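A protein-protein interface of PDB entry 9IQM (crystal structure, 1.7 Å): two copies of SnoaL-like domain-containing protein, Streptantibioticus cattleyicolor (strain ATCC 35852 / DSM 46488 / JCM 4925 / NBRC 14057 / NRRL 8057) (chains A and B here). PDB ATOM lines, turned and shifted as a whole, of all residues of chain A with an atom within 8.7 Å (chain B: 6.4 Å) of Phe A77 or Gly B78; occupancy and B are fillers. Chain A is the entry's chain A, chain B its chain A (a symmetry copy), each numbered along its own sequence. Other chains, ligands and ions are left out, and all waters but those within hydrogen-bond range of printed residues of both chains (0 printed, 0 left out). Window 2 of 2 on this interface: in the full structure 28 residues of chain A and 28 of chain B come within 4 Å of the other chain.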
ATOM      1  N   ALA A   3      23.754 -13.042  23.096  1.00  0.00           N
ATOM      2  CA  ALA A   3      23.289 -11.659  23.117  1.00  0.00           C
ATOM      3  C   ALA A   3      22.475 -11.326  24.362  1.00  0.00           C
ATOM      4  O   ALA A   3      21.854 -10.259  24.420  1.00  0.00           O
ATOM      5  CB  ALA A   3      22.473 -11.315  21.863  1.00  0.00           C
ATOM      6  N   ILE A   6      22.926  -7.866  25.795  1.00  0.00           N
ATOM      7  CA  ILE A   6      22.212  -6.736  25.220  1.00  0.00           C
ATOM      8  C   ILE A   6      20.871  -6.558  25.927  1.00  0.00           C
ATOM      9  O   ILE A   6      20.490  -5.446  26.300  1.00  0.00           O
ATOM     10  CB  ILE A   6      22.036  -6.919  23.706  1.00  0.00           C
ATOM     11  CG1 ILE A   6      23.399  -6.991  23.028  1.00  0.00           C
ATOM     12  CG2 ILE A   6      21.236  -5.750  23.114  1.00  0.00           C
ATOM     13  CD1 ILE A   6      23.295  -7.344  21.562  1.00  0.00           C
ATOM     14  N   PRO A  74      17.272  -7.244  18.863  1.00  0.00           N
ATOM     15  CA  PRO A  74      18.528  -7.202  18.098  1.00  0.00           C
ATOM     16  C   PRO A  74      18.536  -8.180  16.943  1.00  0.00           C
ATOM     17  O   PRO A  74      18.094  -9.325  17.061  1.00  0.00           O
ATOM     18  CB  PRO A  74      19.603  -7.573  19.127  1.00  0.00           C
ATOM     19  CG  PRO A  74      18.876  -8.147  20.280  1.00  0.00           C
ATOM     20  CD  PRO A  74      17.510  -7.494  20.292  1.00  0.00           C
ATOM     21  N   ILE A  75      19.082  -7.723  15.825  1.00  0.00           N
ATOM     22  CA  ILE A  75      19.389  -8.598  14.704  1.00  0.00           C
ATOM     23  C   ILE A  75      20.850  -8.995  14.881  1.00  0.00           C
ATOM     24  O   ILE A  75      21.742  -8.143  14.846  1.00  0.00           O
ATOM     25  CB  ILE A  75      19.150  -7.901  13.360  1.00  0.00           C
ATOM     26  CG1 ILE A  75      17.758  -7.263  13.309  1.00  0.00           C
ATOM     27  CG2 ILE A  75      19.373  -8.868  12.196  1.00  0.00           C
ATOM     28  CD1 ILE A  75      16.626  -8.255  13.371  1.00  0.00           C
ATOM     29  N   MET A  76      21.093 -10.272  15.137  1.00  0.00           N
ATOM     30  CA  MET A  76      22.440 -10.793  15.330  1.00  0.00           C
ATOM     31  C   MET A  76      23.096 -11.194  14.023  1.00  0.00           C
ATOM     32  O   MET A  76      22.515 -11.935  13.232  1.00  0.00           O
ATOM     33  CB  MET A  76      22.401 -11.998  16.278  1.00  0.00           C
ATOM     34  CG  MET A  76      21.711 -11.744  17.606  1.00  0.00           C
ATOM     35  SD  MET A  76      22.344 -10.287  18.482  1.00  0.00           S
ATOM     36  CE  MET A  76      24.022 -10.842  18.880  1.00  0.00           C
ATOM     37  N   PHE A  77      24.338 -10.762  13.838  1.00  0.00           N
ATOM     38  CA  PHE A  77      25.083 -11.166  12.658  1.00  0.00           C
ATOM     39  C   PHE A  77      26.269 -12.046  13.018  1.00  0.00           C
ATOM     40  O   PHE A  77      26.355 -13.185  12.544  1.00  0.00           O
ATOM     41  CB  PHE A  77      25.509  -9.927  11.867  1.00  0.00           C
ATOM     42  CG  PHE A  77      24.350  -9.200  11.265  1.00  0.00           C
ATOM     43  CD1 PHE A  77      23.841  -9.570  10.032  1.00  0.00           C
ATOM     44  CD2 PHE A  77      23.733  -8.174  11.949  1.00  0.00           C
ATOM     45  CE1 PHE A  77      22.751  -8.895   9.492  1.00  0.00           C
ATOM     46  CE2 PHE A  77      22.660  -7.506  11.412  1.00  0.00           C
ATOM     47  CZ  PHE A  77      22.162  -7.870  10.187  1.00  0.00           C
ATOM     48  N   GLY A  78      27.175 -11.571  13.858  1.00  0.00           N
ATOM     49  CA  GLY A  78      28.337 -12.415  14.061  1.00  0.00           C
ATOM     50  C   GLY A  78      28.257 -13.437  15.176  1.00  0.00           C
ATOM     51  O   GLY A  78      29.259 -14.110  15.434  1.00  0.00           O
ATOM     52  N   GLU A  79      27.112 -13.576  15.852  1.00  0.00           N
ATOM     53  CA  GLU A  79      27.087 -14.167  17.189  1.00  0.00           C
ATOM     54  C   GLU A  79      27.692 -13.162  18.169  1.00  0.00           C
ATOM     55  O   GLU A  79      27.318 -13.119  19.345  1.00  0.00           O
ATOM     56  CB  GLU A  79      27.839 -15.503  17.222  1.00  0.00           C
ATOM     57  CG  GLU A  79      27.795 -16.263  18.554  1.00  0.00           C
ATOM     58  CD  GLU A  79      26.629 -17.230  18.668  1.00  0.00           C
ATOM     59  OE1 GLU A  79      26.761 -18.383  18.200  1.00  0.00           O
ATOM     60  OE2 GLU A  79      25.587 -16.850  19.244  1.00  0.00           O
ATOM     61  N   ASN A  80      28.618 -12.335  17.679  1.00  0.00           N
ATOM     62  CA  ASN A  80      29.280 -11.297  18.457  1.00  0.00           C
ATOM     63  C   ASN A  80      28.845  -9.896  18.062  1.00  0.00           C
ATOM     64  O   ASN A  80      29.445  -8.920  18.526  1.00  0.00           O
ATOM     65  CB  ASN A  80      30.799 -11.397  18.311  1.00  0.00           C
ATOM     66  CG  ASN A  80      31.432 -12.247  19.386  1.00  0.00           C
ATOM     67  OD1 ASN A  80      30.823 -12.504  20.432  1.00  0.00           O
ATOM     68  ND2 ASN A  80      32.658 -12.698  19.136  1.00  0.00           N
ATOM     69  N   MET A  81      27.839  -9.771  17.206  1.00  0.00           N
ATOM     70  CA  MET A  81      27.451  -8.470  16.690  1.00  0.00           C
ATOM     71  C   MET A  81      25.940  -8.398  16.635  1.00  0.00           C
ATOM     72  O   MET A  81      25.298  -9.283  16.073  1.00  0.00           O
ATOM     73  CB  MET A  81      28.027  -8.253  15.297  1.00  0.00           C
ATOM     74  CG  MET A  81      27.985  -6.855  14.813  1.00  0.00           C
ATOM     75  SD  MET A  81      26.383  -6.446  14.104  1.00  0.00           S
ATOM     76  CE  MET A  81      26.395  -4.679  14.404  1.00  0.00           C
ATOM     77  N   GLY A  82      25.381  -7.338  17.192  1.00  0.00           N
ATOM     78  CA  GLY A  82      23.940  -7.166  17.214  1.00  0.00           C
ATOM     79  C   GLY A  82      23.578  -5.770  16.772  1.00  0.00           C
ATOM     80  O   GLY A  82      24.223  -4.801  17.188  1.00  0.00           O
ATOM     81  N   LEU A  83      22.583  -5.652  15.912  1.00  0.00           N
ATOM     82  CA  LEU A  83      22.119  -4.356  15.425  1.00  0.00           C
ATOM     83  C   LEU A  83      20.738  -4.135  16.015  1.00  0.00           C
ATOM     84  O   LEU A  83      19.847  -4.964  15.797  1.00  0.00           O
ATOM     85  CB  LEU A  83      22.073  -4.359  13.899  1.00  0.00           C
ATOM     86  CG  LEU A  83      21.179  -3.353  13.175  1.00  0.00           C
ATOM     87  CD1 LEU A  83      21.918  -2.061  13.006  1.00  0.00           C
ATOM     88  CD2 LEU A  83      20.720  -3.923  11.817  1.00  0.00           C
ATOM     89  N   VAL A  84      20.582  -3.080  16.818  1.00  0.00           N
ATOM     90  CA  VAL A  84      19.305  -2.719  17.424  1.00  0.00           C
ATOM     91  C   VAL A  84      18.822  -1.463  16.718  1.00  0.00           C
ATOM     92  O   VAL A  84      19.416  -0.392  16.874  1.00  0.00           O
ATOM     93  CB  VAL A  84      19.432  -2.482  18.933  1.00  0.00           C
ATOM     94  CG1 VAL A  84      18.128  -1.879  19.505  1.00  0.00           C
ATOM     95  CG2 VAL A  84      19.763  -3.790  19.636  1.00  0.00           C
ATOM     96  N   ARG A  85      17.763  -1.595  15.926  1.00  0.00           N
ATOM     97  CA  ARG A  85      17.156  -0.435  15.285  1.00  0.00           C
ATOM     98  C   ARG A  85      16.242   0.271  16.266  1.00  0.00           C
ATOM     99  O   ARG A  85      15.635  -0.356  17.137  1.00  0.00           O
ATOM    100  CB  ARG A  85      16.369  -0.849  14.044  1.00  0.00           C
ATOM    101  CG  ARG A  85      17.277  -1.246  12.867  1.00  0.00           C
ATOM    102  CD  ARG A  85      16.491  -1.381  11.552  1.00  0.00           C
ATOM    103  NE  ARG A  85      17.373  -1.633  10.410  1.00  0.00           N
ATOM    104  CZ  ARG A  85      18.138  -0.717   9.820  1.00  0.00           C
ATOM    105  NH1 ARG A  85      18.126   0.548  10.198  1.00  0.00           N
ATOM    106  NH2 ARG A  85      18.927  -1.084   8.810  1.00  0.00           N
ATOM    107  N   ASP A 101      21.739   1.158  17.005  1.00  0.00           N
ATOM    108  CA  ASP A 101      22.782   0.827  17.973  1.00  0.00           C
ATOM    109  C   ASP A 101      23.518  -0.399  17.465  1.00  0.00           C
ATOM    110  O   ASP A 101      22.895  -1.437  17.274  1.00  0.00           O
ATOM    111  CB  ASP A 101      22.215   0.498  19.360  1.00  0.00           C
ATOM    112  CG  ASP A 101      21.534   1.649  20.038  1.00  0.00           C
ATOM    113  OD1 ASP A 101      21.488   2.760  19.494  1.00  0.00           O
ATOM    114  OD2 ASP A 101      20.985   1.398  21.138  1.00  0.00           O
ATOM    115  N   LEU A 102      24.811  -0.277  17.242  1.00  0.00           N
ATOM    116  CA  LEU A 102      25.639  -1.425  16.907  1.00  0.00           C
ATOM    117  C   LEU A 102      26.299  -1.932  18.178  1.00  0.00           C
ATOM    118  O   LEU A 102      27.012  -1.183  18.843  1.00  0.00           O
ATOM    119  CB  LEU A 102      26.689  -1.048  15.865  1.00  0.00           C
ATOM    120  CG  LEU A 102      26.043  -0.300  14.701  1.00  0.00           C
ATOM    121  CD1 LEU A 102      27.094   0.176  13.710  1.00  0.00           C
ATOM    122  CD2 LEU A 102      24.990  -1.164  14.037  1.00  0.00           C
ATOM    123  N   PHE A 103      26.060  -3.195  18.526  1.00  0.00           N
ATOM    124  CA  PHE A 103      26.695  -3.805  19.688  1.00  0.00           C
ATOM    125  C   PHE A 103      27.752  -4.776  19.192  1.00  0.00           C
ATOM    126  O   PHE A 103      27.448  -5.651  18.371  1.00  0.00           O
ATOM    127  CB  PHE A 103      25.674  -4.533  20.574  1.00  0.00           C
ATOM    128  CG  PHE A 103      24.764  -3.611  21.339  1.00  0.00           C
ATOM    129  CD1 PHE A 103      23.591  -3.117  20.760  1.00  0.00           C
ATOM    130  CD2 PHE A 103      25.063  -3.235  22.642  1.00  0.00           C
ATOM    131  CE1 PHE A 103      22.740  -2.294  21.467  1.00  0.00           C
ATOM    132  CE2 PHE A 103      24.217  -2.388  23.346  1.00  0.00           C
ATOM    133  CZ  PHE A 103      23.054  -1.914  22.760  1.00  0.00           C
ATOM    134  N   ILE A 104      28.994  -4.609  19.653  1.00  0.00           N
ATOM    135  CA  ILE A 104      30.042  -5.609  19.483  1.00  0.00           C
ATOM    136  C   ILE A 104      30.239  -6.281  20.830  1.00  0.00           C
ATOM    137  O   ILE A 104      30.402  -5.602  21.860  1.00  0.00           O
ATOM    138  CB  ILE A 104      31.362  -5.000  18.983  1.00  0.00           C
ATOM    139  CG1 ILE A 104      31.162  -4.367  17.606  1.00  0.00           C
ATOM    140  CG2 ILE A 104      32.414  -6.098  18.875  1.00  0.00           C
ATOM    141  CD1 ILE A 104      30.678  -5.327  16.556  1.00  0.00           C
ATOM    142  N   MET B  76      33.465  -7.935   8.090  1.00  0.00           N
ATOM    143  CA  MET B  76      32.378  -8.879   7.867  1.00  0.00           C
ATOM    144  C   MET B  76      31.909  -9.533   9.153  1.00  0.00           C
ATOM    145  O   MET B  76      32.714 -10.060   9.916  1.00  0.00           O
ATOM    146  CB  MET B  76      32.821  -9.958   6.872  1.00  0.00           C
ATOM    147  CG  MET B  76      33.374  -9.430   5.560  1.00  0.00           C
ATOM    148  SD  MET B  76      32.272  -8.245   4.738  1.00  0.00           S
ATOM    149  CE  MET B  76      30.883  -9.326   4.307  1.00  0.00           C
ATOM    150  N   PHE B  77      30.595  -9.561   9.346  1.00  0.00           N
ATOM    151  CA  PHE B  77      30.043 -10.243  10.503  1.00  0.00           C
ATOM    152  C   PHE B  77      29.229 -11.461  10.100  1.00  0.00           C
ATOM    153  O   PHE B  77      29.542 -12.579  10.528  1.00  0.00           O
ATOM    154  CB  PHE B  77      29.223  -9.258  11.339  1.00  0.00           C
ATOM    155  CG  PHE B  77      30.065  -8.202  11.979  1.00  0.00           C
ATOM    156  CD1 PHE B  77      30.680  -8.424  13.199  1.00  0.00           C
ATOM    157  CD2 PHE B  77      30.288  -7.000  11.341  1.00  0.00           C
ATOM    158  CE1 PHE B  77      31.476  -7.437  13.774  1.00  0.00           C
ATOM    159  CE2 PHE B  77      31.071  -6.026  11.910  1.00  0.00           C
ATOM    160  CZ  PHE B  77      31.671  -6.246  13.125  1.00  0.00           C
ATOM    161  N   GLY B  78      28.209 -11.294   9.273  1.00  0.00           N
ATOM    162  CA  GLY B  78      27.406 -12.476   9.028  1.00  0.00           C
ATOM    163  C   GLY B  78      27.824 -13.364   7.873  1.00  0.00           C
ATOM    164  O   GLY B  78      27.112 -14.329   7.583  1.00  0.00           O
ATOM    165  N   GLU B  79      28.942 -13.074   7.202  1.00  0.00           N
ATOM    166  CA  GLU B  79      29.159 -13.566   5.842  1.00  0.00           C
ATOM    167  C   GLU B  79      28.239 -12.792   4.898  1.00  0.00           C
ATOM    168  O   GLU B  79      28.567 -12.576   3.727  1.00  0.00           O
ATOM    169  CB  GLU B  79      28.911 -15.077   5.750  1.00  0.00           C
ATOM    170  CG  GLU B  79      29.204 -15.722   4.389  1.00  0.00           C
ATOM    171  CD  GLU B  79      30.631 -16.224   4.245  1.00  0.00           C
ATOM    172  OE1 GLU B  79      30.906 -17.370   4.665  1.00  0.00           O
ATOM    173  OE2 GLU B  79      31.475 -15.486   3.691  1.00  0.00           O
ATOM    174  N   ASN B  80      27.088 -12.353   5.414  1.00  0.00           N
ATOM    175  CA  ASN B  80      26.105 -11.576   4.674  1.00  0.00           C
ATOM    176  C   ASN B  80      26.036 -10.128   5.127  1.00  0.00           C
ATOM    177  O   ASN B  80      25.133  -9.399   4.699  1.00  0.00           O
ATOM    178  CB  ASN B  80      24.714 -12.197   4.805  1.00  0.00           C
ATOM    179  CG  ASN B  80      24.404 -13.168   3.692  1.00  0.00           C
ATOM    180  OD1 ASN B  80      25.056 -13.159   2.641  1.00  0.00           O
ATOM    181  ND2 ASN B  80      23.409 -14.023   3.915  1.00  0.00           N
ATOM    182  N   MET B  81      26.943  -9.698   5.995  1.00  0.00           N
ATOM    183  CA  MET B  81      26.865  -8.366   6.565  1.00  0.00           C
ATOM    184  C   MET B  81      28.259  -7.781   6.634  1.00  0.00           C
ATOM    185  O   MET B  81      29.170  -8.414   7.165  1.00  0.00           O
ATOM    186  CB  MET B  81      26.258  -8.416   7.962  1.00  0.00           C
ATOM    187  CG  MET B  81      25.822  -7.108   8.501  1.00  0.00           C
ATOM    188  SD  MET B  81      27.191  -6.203   9.237  1.00  0.00           S
ATOM    189  CE  MET B  81      26.570  -4.536   9.008  1.00  0.00           C
ATOM    190  N   GLY B  82      28.417  -6.572   6.123  1.00  0.00           N
ATOM    191  CA  GLY B  82      29.710  -5.915   6.118  1.00  0.00           C
ATOM    192  C   GLY B  82      29.575  -4.498   6.618  1.00  0.00           C
ATOM    193  O   GLY B  82      28.633  -3.794   6.237  1.00  0.00           O
ATOM    194  N   PHE B 103      26.347  -2.865   4.951  1.00  0.00           N
ATOM    195  CA  PHE B 103      25.952  -3.608   3.761  1.00  0.00           C
ATOM    196  C   PHE B 103      25.296  -4.903   4.210  1.00  0.00           C
ATOM    197  O   PHE B 103      25.887  -5.652   4.998  1.00  0.00           O
ATOM    198  CB  PHE B 103      27.154  -3.906   2.854  1.00  0.00           C
ATOM    199  CG  PHE B 103      27.686  -2.698   2.133  1.00  0.00           C
ATOM    200  CD1 PHE B 103      28.623  -1.855   2.740  1.00  0.00           C
ATOM    201  CD2 PHE B 103      27.268  -2.396   0.843  1.00  0.00           C
ATOM    202  CE1 PHE B 103      29.135  -0.762   2.072  1.00  0.00           C
ATOM    203  CE2 PHE B 103      27.766  -1.282   0.180  1.00  0.00           C
ATOM    204  CZ  PHE B 103      28.700  -0.461   0.793  1.00  0.00           C
ATOM    205  N   ILE B 104      24.069  -5.153   3.747  1.00  0.00           N
ATOM    206  CA  ILE B 104      23.429  -6.459   3.871  1.00  0.00           C
ATOM    207  C   ILE B 104      23.466  -7.104   2.496  1.00  0.00           C
ATOM    208  O   ILE B 104      23.072  -6.481   1.493  1.00  0.00           O
ATOM    209  CB  ILE B 104      21.983  -6.361   4.385  1.00  0.00           C
ATOM    210  CG1 ILE B 104      21.963  -5.753   5.788  1.00  0.00           C
ATOM    211  CG2 ILE B 104      21.374  -7.757   4.442  1.00  0.00           C
ATOM    212  CD1 ILE B 104      22.755  -6.530   6.802  1.00  0.00           C
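Phe A77 touches its own counterpart, Phe B77.
Phe A77 touches Gly B78, and with the chains exchanged Gly A78 touches Phe B77.
Phe A77 touches Met B81, and with the chains exchanged Met A81 touches Phe B77.
Phe A77 touches Ile B104, and with the chains exchanged Ile A104 touches Phe B77.
Positions printed for both chains: 76, 77, 78, 79, 80, 81, 82, 103 and 104.
Of the 7 pairs that touch across the chains among the printed residues, 7 have their exchanged pair printed and touching as well.
Among the printed residues, pairs that only touch across the chains: Phe A77 with Met B81, Met A81 with Phe B77, Ile A104 with Phe B77, Phe A77 with Ile B104, Gly A78 with Phe B77, Phe A77 with Gly B78 and Phe A77 with Phe B77.
Of chain B, only Phe B77 (3.8 Å), Gly B78 (3.7 Å), Met B81 (3.4 Å) and Ile B104 (3.6 Å) come within 4 Å of Phe A77.
Of the printed residues of chain B, Met A81 touches Phe B77.
Gly A82 touches none of the printed residues of chain B.
Of the printed residues of chain A, Phe B77 touches Phe A77, Gly A78, Met A81 and Ile A104.
Gly B78 touches just one residue of chain A: Phe A77.
Printed residues of chain A within 4 Å of Met B81: Phe A77.
Of the printed residues of chain A, Ile B104 touches Phe A77 (3.6 Å).
The nearest residue of chain B that does not touch Phe A77 is Asn B80 (5.4 Å).
The nearest residue of chain A that does not touch Gly B78 is Gly A78 (4.7 Å).
The nearest printed residue of chain B that does not touch Gly A78 is Gly B78 (4.7 Å).
Of the 18 printed residues of chain A, 4 touch a printed residue of chain B.
Hydrophobic or aromatic side chains of chain A within 4 Å of the printed part of chain B: Phe A77, Met A81 and Ile A104.
Among the printed residues, no Asp or Glu carboxylate lies within 4 Å of a Lys or Arg side-chain nitrogen of the other chain.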
